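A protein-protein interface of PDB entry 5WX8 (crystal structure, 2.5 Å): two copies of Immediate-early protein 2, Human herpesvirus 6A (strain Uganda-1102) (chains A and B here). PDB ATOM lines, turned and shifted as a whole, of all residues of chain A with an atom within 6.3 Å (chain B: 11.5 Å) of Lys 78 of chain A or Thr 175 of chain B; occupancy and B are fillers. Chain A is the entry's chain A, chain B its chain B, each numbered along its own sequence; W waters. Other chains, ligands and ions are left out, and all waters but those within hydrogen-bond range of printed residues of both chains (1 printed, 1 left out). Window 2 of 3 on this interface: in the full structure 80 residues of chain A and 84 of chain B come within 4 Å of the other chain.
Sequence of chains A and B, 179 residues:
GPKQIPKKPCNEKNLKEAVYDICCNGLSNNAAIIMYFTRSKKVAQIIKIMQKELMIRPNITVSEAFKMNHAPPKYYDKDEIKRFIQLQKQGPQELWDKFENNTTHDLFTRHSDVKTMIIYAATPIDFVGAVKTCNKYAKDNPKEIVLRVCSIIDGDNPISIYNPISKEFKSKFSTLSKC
OD1 of Asp 77 of chain A is in hydrogen-bond range of N of Glu 80 of chain A (3.0 Å). The side-chain hydroxyl of Thr 123 of chain B lies close to the backbone NH of Ile 125 of chain B (3.1 Å). The side-chain amino group (NZ) of Lys 172 of chain B is in salt-bridge range of the side-chain carboxylate (OE1) of Glu 168 of chain B (3.8 Å).
OG1 of Thr 123 of chain B touches CE2 of Tyr 76 of chain A, at 3.6 Å. Tyr 76 of chain A touches Ile 125 of chain B. CE of Lys 78 of chain A touches NZ of Lys 172 of chain B, 3.7 Å away. Thr 175 of chain B touches Lys 78 of chain A (CG2 to NZ, 3.3 Å). Leu 176 of chain B touches Lys 78 of chain A. Glu 80 of chain A touches Ile 125 of chain B. Ile 81 of chain A touches Phe 169 of chain B. CD1 of Ile 81 of chain A touches CB of Lys 172 of chain B, at 3.6 Å. Leu 176 of chain B touches Lys 82 of chain A.
No residue of chain B comes within 4 Å of Asp 77 of chain A. Lys 78 of chain A touches three residues of chain B. No residue of chain B comes within 4 Å of Asp 79 of chain A. Of the printed residues of chain B, Glu 80 of chain A touches Ile 125 (3.8 Å). Cys 24 of chain B touches none of the printed residues of chain A. Asn 25 of chain B touches none of the printed residues of chain A. Of the printed residues of chain A, Thr 123 of chain B touches Tyr 76. Of the printed residues of chain A, Phe 169 of chain B touches Ile 81. Thr 175 of chain B touches one residue of chain A. Of the printed residues of chain A, Leu 176 of chain B touches Lys 78 and Lys 82. The nearest residue of chain B that does not touch Lys 78 of chain A is Ser 171 of chain B (5.2 Å). The nearest printed residue of chain A that does not touch Thr 175 of chain B is Ile 81 of chain A (7.8 Å).
Hydrophobic or aromatic side chains of chain A within 4 Å of the printed part of chain B: Tyr 76 and Ile 81. Along chain A the printed residues that touch a printed residue of chain B span positions 76 to 82. Printed residues of chain B that touch a printed residue of chain A: Thr 123, Ile 125, Phe 169, Lys 172, Thr 175 and Leu 176. Hydrophobic or aromatic side chains of chain B that line the printed part of chain A: Ile 125, Phe 169 and Leu 176. Among the printed residues, no Asp or Glu carboxylate lies within 4 Å of a Lys or Arg side-chain nitrogen of the other chain.
No position is printed for both chains. Of the 9 pairs that touch across the chains among the printed residues, none has its exchanged pair printed and touching as well.
Water W1 lies within hydrogen-bond range of the backbone NH (N) of Tyr 76 of chain A (3.1 Å) and the backbone carbonyl oxygen (O) of Ile 165 of chain B (3.2 Å).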
ATOM      1  N   TYR A  76     -35.125   6.677 -28.349  1.00  0.00           N
ATOM      2  CA  TYR A  76     -34.551   5.465 -28.920  1.00  0.00           C
ATOM      3  C   TYR A  76     -34.408   4.417 -27.827  1.00  0.00           C
ATOM      4  O   TYR A  76     -34.022   4.738 -26.699  1.00  0.00           O
ATOM      5  CB  TYR A  76     -33.193   5.740 -29.575  1.00  0.00           C
ATOM      6  CG  TYR A  76     -33.326   6.431 -30.905  1.00  0.00           C
ATOM      7  CD1 TYR A  76     -33.856   5.769 -31.989  1.00  0.00           C
ATOM      8  CD2 TYR A  76     -32.942   7.765 -31.071  1.00  0.00           C
ATOM      9  CE1 TYR A  76     -34.002   6.400 -33.211  1.00  0.00           C
ATOM     10  CE2 TYR A  76     -33.093   8.420 -32.300  1.00  0.00           C
ATOM     11  CZ  TYR A  76     -33.630   7.726 -33.362  1.00  0.00           C
ATOM     12  OH  TYR A  76     -33.789   8.318 -34.586  1.00  0.00           O
ATOM     13  N   ASP A  77     -34.734   3.166 -28.158  1.00  0.00           N
ATOM     14  CA  ASP A  77     -34.707   2.118 -27.147  1.00  0.00           C
ATOM     15  C   ASP A  77     -33.294   1.531 -27.011  1.00  0.00           C
ATOM     16  O   ASP A  77     -32.391   1.806 -27.814  1.00  0.00           O
ATOM     17  CB  ASP A  77     -35.759   1.036 -27.444  1.00  0.00           C
ATOM     18  CG  ASP A  77     -35.441   0.178 -28.683  1.00  0.00           C
ATOM     19  OD1 ASP A  77     -34.326  -0.378 -28.804  1.00  0.00           O
ATOM     20  OD2 ASP A  77     -36.347   0.023 -29.539  1.00  0.00           O
ATOM     21  N   LYS A  78     -33.115   0.711 -25.966  1.00  0.00           N
ATOM     22  CA  LYS A  78     -31.779   0.247 -25.613  1.00  0.00           C
ATOM     23  C   LYS A  78     -31.120  -0.483 -26.776  1.00  0.00           C
ATOM     24  O   LYS A  78     -29.936  -0.263 -27.063  1.00  0.00           O
ATOM     25  CB  LYS A  78     -31.835  -0.639 -24.365  1.00  0.00           C
ATOM     26  CG  LYS A  78     -30.485  -0.765 -23.651  1.00  0.00           C
ATOM     27  CD  LYS A  78     -30.576  -0.945 -22.099  1.00  0.00           C
ATOM     28  CE  LYS A  78     -30.719   0.389 -21.333  1.00  0.00           C
ATOM     29  NZ  LYS A  78     -29.450   0.892 -20.674  1.00  0.00           N
ATOM     30  N   ASP A  79     -31.875  -1.320 -27.491  1.00  0.00           N
ATOM     31  CA  ASP A  79     -31.269  -2.081 -28.580  1.00  0.00           C
ATOM     32  C   ASP A  79     -30.766  -1.165 -29.688  1.00  0.00           C
ATOM     33  O   ASP A  79     -29.642  -1.334 -30.174  1.00  0.00           O
ATOM     34  CB  ASP A  79     -32.253  -3.112 -29.129  1.00  0.00           C
ATOM     35  CG  ASP A  79     -31.923  -4.531 -28.665  1.00  0.00           C
ATOM     36  OD1 ASP A  79     -30.712  -4.857 -28.513  1.00  0.00           O
ATOM     37  OD2 ASP A  79     -32.876  -5.315 -28.440  1.00  0.00           O
ATOM     38  N   GLU A  80     -31.570  -0.174 -30.078  1.00  0.00           N
ATOM     39  CA  GLU A  80     -31.133   0.793 -31.083  1.00  0.00           C
ATOM     40  C   GLU A  80     -29.898   1.563 -30.621  1.00  0.00           C
ATOM     41  O   GLU A  80     -28.981   1.821 -31.417  1.00  0.00           O
ATOM     42  CB  GLU A  80     -32.274   1.758 -31.409  1.00  0.00           C
ATOM     43  CG  GLU A  80     -33.409   1.119 -32.197  1.00  0.00           C
ATOM     44  CD  GLU A  80     -34.644   2.013 -32.337  1.00  0.00           C
ATOM     45  OE1 GLU A  80     -35.161   2.519 -31.302  1.00  0.00           O
ATOM     46  OE2 GLU A  80     -35.086   2.204 -33.500  1.00  0.00           O
ATOM     47  N   ILE A  81     -29.861   1.954 -29.344  1.00  0.00           N
ATOM     48  CA  ILE A  81     -28.700   2.681 -28.848  1.00  0.00           C
ATOM     49  C   ILE A  81     -27.473   1.786 -28.866  1.00  0.00           C
ATOM     50  O   ILE A  81     -26.368   2.242 -29.150  1.00  0.00           O
ATOM     51  CB  ILE A  81     -28.974   3.245 -27.443  1.00  0.00           C
ATOM     52  CG1 ILE A  81     -30.169   4.188 -27.495  1.00  0.00           C
ATOM     53  CG2 ILE A  81     -27.746   3.975 -26.908  1.00  0.00           C
ATOM     54  CD1 ILE A  81     -30.484   4.867 -26.200  1.00  0.00           C
ATOM     55  N   LYS A  82     -27.653   0.493 -28.615  1.00  0.00           N
ATOM     56  CA  LYS A  82     -26.523  -0.425 -28.579  1.00  0.00           C
ATOM     57  C   LYS A  82     -25.913  -0.622 -29.963  1.00  0.00           C
ATOM     58  O   LYS A  82     -24.685  -0.659 -30.110  1.00  0.00           O
ATOM     59  CB  LYS A  82     -26.984  -1.757 -27.995  1.00  0.00           C
ATOM     60  CG  LYS A  82     -25.918  -2.815 -27.881  1.00  0.00           C
ATOM     61  CD  LYS A  82     -26.516  -4.108 -27.328  1.00  0.00           C
ATOM     62  CE  LYS A  82     -27.291  -3.842 -26.043  1.00  0.00           C
ATOM     63  NZ  LYS A  82     -27.495  -5.089 -25.263  1.00  0.00           N
ATOM     64  N   ARG A  83     -26.746  -0.750 -30.990  1.00  0.00           N
ATOM     65  CA  ARG A  83     -26.214  -1.026 -32.319  1.00  0.00           C
ATOM     66  C   ARG A  83     -25.547   0.198 -32.925  1.00  0.00           C
ATOM     67  O   ARG A  83     -24.575   0.061 -33.678  1.00  0.00           O
ATOM     68  CB  ARG A  83     -27.330  -1.560 -33.199  1.00  0.00           C
ATOM     69  CG  ARG A  83     -28.176  -2.504 -32.404  1.00  0.00           C
ATOM     70  CD  ARG A  83     -29.299  -3.052 -33.185  1.00  0.00           C
ATOM     71  NE  ARG A  83     -30.097  -1.977 -33.739  1.00  0.00           N
ATOM     72  CZ  ARG A  83     -31.176  -2.192 -34.468  1.00  0.00           C
ATOM     73  NH1 ARG A  83     -31.540  -3.445 -34.682  1.00  0.00           N
ATOM     74  NH2 ARG A  83     -31.876  -1.176 -34.972  1.00  0.00           N
ATOM     75  N   CYS B  24     -19.013  10.994 -30.203  1.00  0.00           N
ATOM     76  CA  CYS B  24     -18.175  10.055 -29.465  1.00  0.00           C
ATOM     77  C   CYS B  24     -18.703   9.780 -28.063  1.00  0.00           C
ATOM     78  O   CYS B  24     -18.506   8.686 -27.528  1.00  0.00           O
ATOM     79  CB  CYS B  24     -16.746  10.609 -29.400  1.00  0.00           C
ATOM     80  SG  CYS B  24     -15.515   9.465 -28.772  1.00  0.00           S
ATOM     81  N   ASN B  25     -19.397  10.744 -27.466  1.00  0.00           N
ATOM     82  CA  ASN B  25     -19.787  10.655 -26.069  1.00  0.00           C
ATOM     83  C   ASN B  25     -21.298  10.654 -25.873  1.00  0.00           C
ATOM     84  O   ASN B  25     -21.774  10.956 -24.771  1.00  0.00           O
ATOM     85  CB  ASN B  25     -19.139  11.794 -25.284  1.00  0.00           C
ATOM     86  CG  ASN B  25     -17.743  11.431 -24.805  1.00  0.00           C
ATOM     87  OD1 ASN B  25     -16.753  11.682 -25.497  1.00  0.00           O
ATOM     88  ND2 ASN B  25     -17.660  10.818 -23.621  1.00  0.00           N
ATOM     89  N   GLY B  26     -22.062  10.306 -26.908  1.00  0.00           N
ATOM     90  CA  GLY B  26     -23.504  10.194 -26.766  1.00  0.00           C
ATOM     91  C   GLY B  26     -24.239  11.497 -26.554  1.00  0.00           C
ATOM     92  O   GLY B  26     -25.341  11.495 -26.007  1.00  0.00           O
ATOM     93  N   THR B 123     -30.186  13.582 -30.788  1.00  0.00           N
ATOM     94  CA  THR B 123     -29.317  12.489 -30.371  1.00  0.00           C
ATOM     95  C   THR B 123     -28.280  12.192 -31.442  1.00  0.00           C
ATOM     96  O   THR B 123     -28.495  12.469 -32.631  1.00  0.00           O
ATOM     97  CB  THR B 123     -30.082  11.197 -30.081  1.00  0.00           C
ATOM     98  OG1 THR B 123     -30.325  10.508 -31.313  1.00  0.00           O
ATOM     99  CG2 THR B 123     -31.396  11.478 -29.338  1.00  0.00           C
ATOM    100  N   ILE B 125     -27.813   9.517 -32.889  1.00  0.00           N
ATOM    101  CA  ILE B 125     -28.438   8.746 -33.969  1.00  0.00           C
ATOM    102  C   ILE B 125     -29.090   9.675 -34.990  1.00  0.00           C
ATOM    103  O   ILE B 125     -28.959   9.474 -36.205  1.00  0.00           O
ATOM    104  CB  ILE B 125     -29.454   7.741 -33.407  1.00  0.00           C
ATOM    105  CG1 ILE B 125     -28.755   6.545 -32.769  1.00  0.00           C
ATOM    106  CG2 ILE B 125     -30.357   7.267 -34.508  1.00  0.00           C
ATOM    107  CD1 ILE B 125     -29.737   5.447 -32.367  1.00  0.00           C
ATOM    108  N   ILE B 165     -35.334  13.650 -24.157  1.00  0.00           N
ATOM    109  CA  ILE B 165     -34.908  12.647 -25.125  1.00  0.00           C
ATOM    110  C   ILE B 165     -33.390  12.561 -25.160  1.00  0.00           C
ATOM    111  O   ILE B 165     -32.823  11.468 -25.154  1.00  0.00           O
ATOM    112  CB  ILE B 165     -35.496  12.946 -26.516  1.00  0.00           C
ATOM    113  CG1 ILE B 165     -36.990  12.587 -26.541  1.00  0.00           C
ATOM    114  CG2 ILE B 165     -34.714  12.204 -27.606  1.00  0.00           C
ATOM    115  CD1 ILE B 165     -37.909  13.602 -25.803  1.00  0.00           C
ATOM    116  N   SER B 166     -32.710  13.704 -25.167  1.00  0.00           N
ATOM    117  CA  SER B 166     -31.256  13.689 -25.076  1.00  0.00           C
ATOM    118  C   SER B 166     -30.775  13.092 -23.757  1.00  0.00           C
ATOM    119  O   SER B 166     -29.810  12.321 -23.742  1.00  0.00           O
ATOM    120  CB  SER B 166     -30.717  15.102 -25.240  1.00  0.00           C
ATOM    121  OG  SER B 166     -31.372  15.741 -26.311  1.00  0.00           O
ATOM    122  N   LYS B 167     -31.412  13.450 -22.635  1.00  0.00           N
ATOM    123  CA  LYS B 167     -30.926  12.958 -21.343  1.00  0.00           C
ATOM    124  C   LYS B 167     -31.152  11.458 -21.197  1.00  0.00           C
ATOM    125  O   LYS B 167     -30.349  10.762 -20.562  1.00  0.00           O
ATOM    126  CB  LYS B 167     -31.602  13.697 -20.186  1.00  0.00           C
ATOM    127  CG  LYS B 167     -31.266  13.112 -18.809  1.00  0.00           C
ATOM    128  CD  LYS B 167     -31.962  13.852 -17.675  1.00  0.00           C
ATOM    129  CE  LYS B 167     -31.608  13.252 -16.296  1.00  0.00           C
ATOM    130  NZ  LYS B 167     -32.784  12.678 -15.551  1.00  0.00           N
ATOM    131  N   GLU B 168     -32.240  10.940 -21.771  1.00  0.00           N
ATOM    132  CA  GLU B 168     -32.470   9.500 -21.746  1.00  0.00           C
ATOM    133  C   GLU B 168     -31.416   8.761 -22.562  1.00  0.00           C
ATOM    134  O   GLU B 168     -30.828   7.769 -22.105  1.00  0.00           O
ATOM    135  CB  GLU B 168     -33.861   9.207 -22.295  1.00  0.00           C
ATOM    136  CG  GLU B 168     -34.741   8.324 -21.425  1.00  0.00           C
ATOM    137  CD  GLU B 168     -34.500   6.833 -21.630  1.00  0.00           C
ATOM    138  OE1 GLU B 168     -34.865   6.051 -20.728  1.00  0.00           O
ATOM    139  OE2 GLU B 168     -33.964   6.444 -22.692  1.00  0.00           O
ATOM    140  N   PHE B 169     -31.203   9.213 -23.799  1.00  0.00           N
ATOM    141  CA  PHE B 169     -30.208   8.603 -24.675  1.00  0.00           C
ATOM    142  C   PHE B 169     -28.848   8.538 -23.987  1.00  0.00           C
ATOM    143  O   PHE B 169     -28.165   7.509 -24.032  1.00  0.00           O
ATOM    144  CB  PHE B 169     -30.127   9.398 -25.983  1.00  0.00           C
ATOM    145  CG  PHE B 169     -29.246   8.790 -27.027  1.00  0.00           C
ATOM    146  CD1 PHE B 169     -27.866   8.892 -26.944  1.00  0.00           C
ATOM    147  CD2 PHE B 169     -29.795   8.148 -28.114  1.00  0.00           C
ATOM    148  CE1 PHE B 169     -27.058   8.348 -27.898  1.00  0.00           C
ATOM    149  CE2 PHE B 169     -28.993   7.611 -29.091  1.00  0.00           C
ATOM    150  CZ  PHE B 169     -27.615   7.720 -28.989  1.00  0.00           C
ATOM    151  N   LYS B 170     -28.451   9.634 -23.328  1.00  0.00           N
ATOM    152  CA  LYS B 170     -27.153   9.676 -22.661  1.00  0.00           C
ATOM    153  C   LYS B 170     -27.090   8.682 -21.502  1.00  0.00           C
ATOM    154  O   LYS B 170     -26.103   7.955 -21.357  1.00  0.00           O
ATOM    155  CB  LYS B 170     -26.863  11.095 -22.182  1.00  0.00           C
ATOM    156  CG  LYS B 170     -25.603  11.233 -21.355  1.00  0.00           C
ATOM    157  CD  LYS B 170     -24.351  10.913 -22.155  1.00  0.00           C
ATOM    158  CE  LYS B 170     -23.112  11.017 -21.272  1.00  0.00           C
ATOM    159  NZ  LYS B 170     -21.980  10.223 -21.830  1.00  0.00           N
ATOM    160  N   SER B 171     -28.132   8.646 -20.663  1.00  0.00           N
ATOM    161  CA  SER B 171     -28.245   7.647 -19.598  1.00  0.00           C
ATOM    162  C   SER B 171     -28.017   6.240 -20.133  1.00  0.00           C
ATOM    163  O   SER B 171     -27.191   5.483 -19.604  1.00  0.00           O
ATOM    164  CB  SER B 171     -29.630   7.711 -18.938  1.00  0.00           C
ATOM    165  OG  SER B 171     -29.787   8.847 -18.111  1.00  0.00           O
ATOM    166  N   LYS B 172     -28.761   5.867 -21.173  1.00  0.00           N
ATOM    167  CA  LYS B 172     -28.648   4.510 -21.692  1.00  0.00           C
ATOM    168  C   LYS B 172     -27.278   4.286 -22.308  1.00  0.00           C
ATOM    169  O   LYS B 172     -26.667   3.220 -22.127  1.00  0.00           O
ATOM    170  CB  LYS B 172     -29.754   4.250 -22.717  1.00  0.00           C
ATOM    171  CG  LYS B 172     -31.131   3.984 -22.120  1.00  0.00           C
ATOM    172  CD  LYS B 172     -32.108   3.516 -23.194  1.00  0.00           C
ATOM    173  CE  LYS B 172     -33.551   3.490 -22.694  1.00  0.00           C
ATOM    174  NZ  LYS B 172     -33.683   2.563 -21.528  1.00  0.00           N
ATOM    175  N   PHE B 173     -26.774   5.300 -23.017  1.00  0.00           N
ATOM    176  CA  PHE B 173     -25.491   5.187 -23.699  1.00  0.00           C
ATOM    177  C   PHE B 173     -24.357   4.982 -22.699  1.00  0.00           C
ATOM    178  O   PHE B 173     -23.445   4.187 -22.948  1.00  0.00           O
ATOM    179  CB  PHE B 173     -25.276   6.434 -24.572  1.00  0.00           C
ATOM    180  CG  PHE B 173     -23.962   6.470 -25.309  1.00  0.00           C
ATOM    181  CD1 PHE B 173     -22.817   6.983 -24.708  1.00  0.00           C
ATOM    182  CD2 PHE B 173     -23.876   6.019 -26.618  1.00  0.00           C
ATOM    183  CE1 PHE B 173     -21.612   7.033 -25.390  1.00  0.00           C
ATOM    184  CE2 PHE B 173     -22.669   6.062 -27.305  1.00  0.00           C
ATOM    185  CZ  PHE B 173     -21.539   6.572 -26.691  1.00  0.00           C
ATOM    186  N   SER B 174     -24.395   5.680 -21.557  1.00  0.00           N
ATOM    187  CA  SER B 174     -23.344   5.478 -20.564  1.00  0.00           C
ATOM    188  C   SER B 174     -23.449   4.111 -19.889  1.00  0.00           C
ATOM    189  O   SER B 174     -22.425   3.534 -19.506  1.00  0.00           O
ATOM    190  CB  SER B 174     -23.372   6.599 -19.537  1.00  0.00           C
ATOM    191  OG  SER B 174     -22.649   7.706 -20.026  1.00  0.00           O
ATOM    192  N   THR B 175     -24.661   3.564 -19.754  1.00  0.00           N
ATOM    193  CA  THR B 175     -24.812   2.189 -19.278  1.00  0.00           C
ATOM    194  C   THR B 175     -24.283   1.179 -20.295  1.00  0.00           C
ATOM    195  O   THR B 175     -23.721   0.146 -19.919  1.00  0.00           O
ATOM    196  CB  THR B 175     -26.282   1.909 -18.948  1.00  0.00           C
ATOM    197  OG1 THR B 175     -26.584   2.416 -17.638  1.00  0.00           O
ATOM    198  CG2 THR B 175     -26.614   0.406 -19.028  1.00  0.00           C
ATOM    199  N   LEU B 176     -24.427   1.459 -21.582  1.00  0.00           N
ATOM    200  CA  LEU B 176     -24.050   0.479 -22.590  1.00  0.00           C
ATOM    201  C   LEU B 176     -22.608   0.603 -23.078  1.00  0.00           C
ATOM    202  O   LEU B 176     -22.156  -0.251 -23.852  1.00  0.00           O
ATOM    203  CB  LEU B 176     -24.994   0.579 -23.784  1.00  0.00           C
ATOM    204  CG  LEU B 176     -26.480   0.403 -23.487  1.00  0.00           C
ATOM    205  CD1 LEU B 176     -27.280   0.615 -24.764  1.00  0.00           C
ATOM    206  CD2 LEU B 176     -26.727  -0.970 -22.902  1.00  0.00           C
ATOM    207  N   SER B 177     -21.873   1.625 -22.661  1.00  0.00           N
ATOM    208  CA  SER B 177     -20.489   1.778 -23.109  1.00  0.00           C
ATOM    209  C   SER B 177     -19.561   0.760 -22.436  1.00  0.00           C
ATOM    210  O   SER B 177     -19.736   0.410 -21.262  1.00  0.00           O
ATOM    211  CB  SER B 177     -19.998   3.211 -22.852  1.00  0.00           C
ATOM    212  OG  SER B 177     -20.688   4.160 -23.669  1.00  0.00           O
HETATM  213  O   HOH W   1     -33.556   8.964 -26.926  1.00  0.00           O
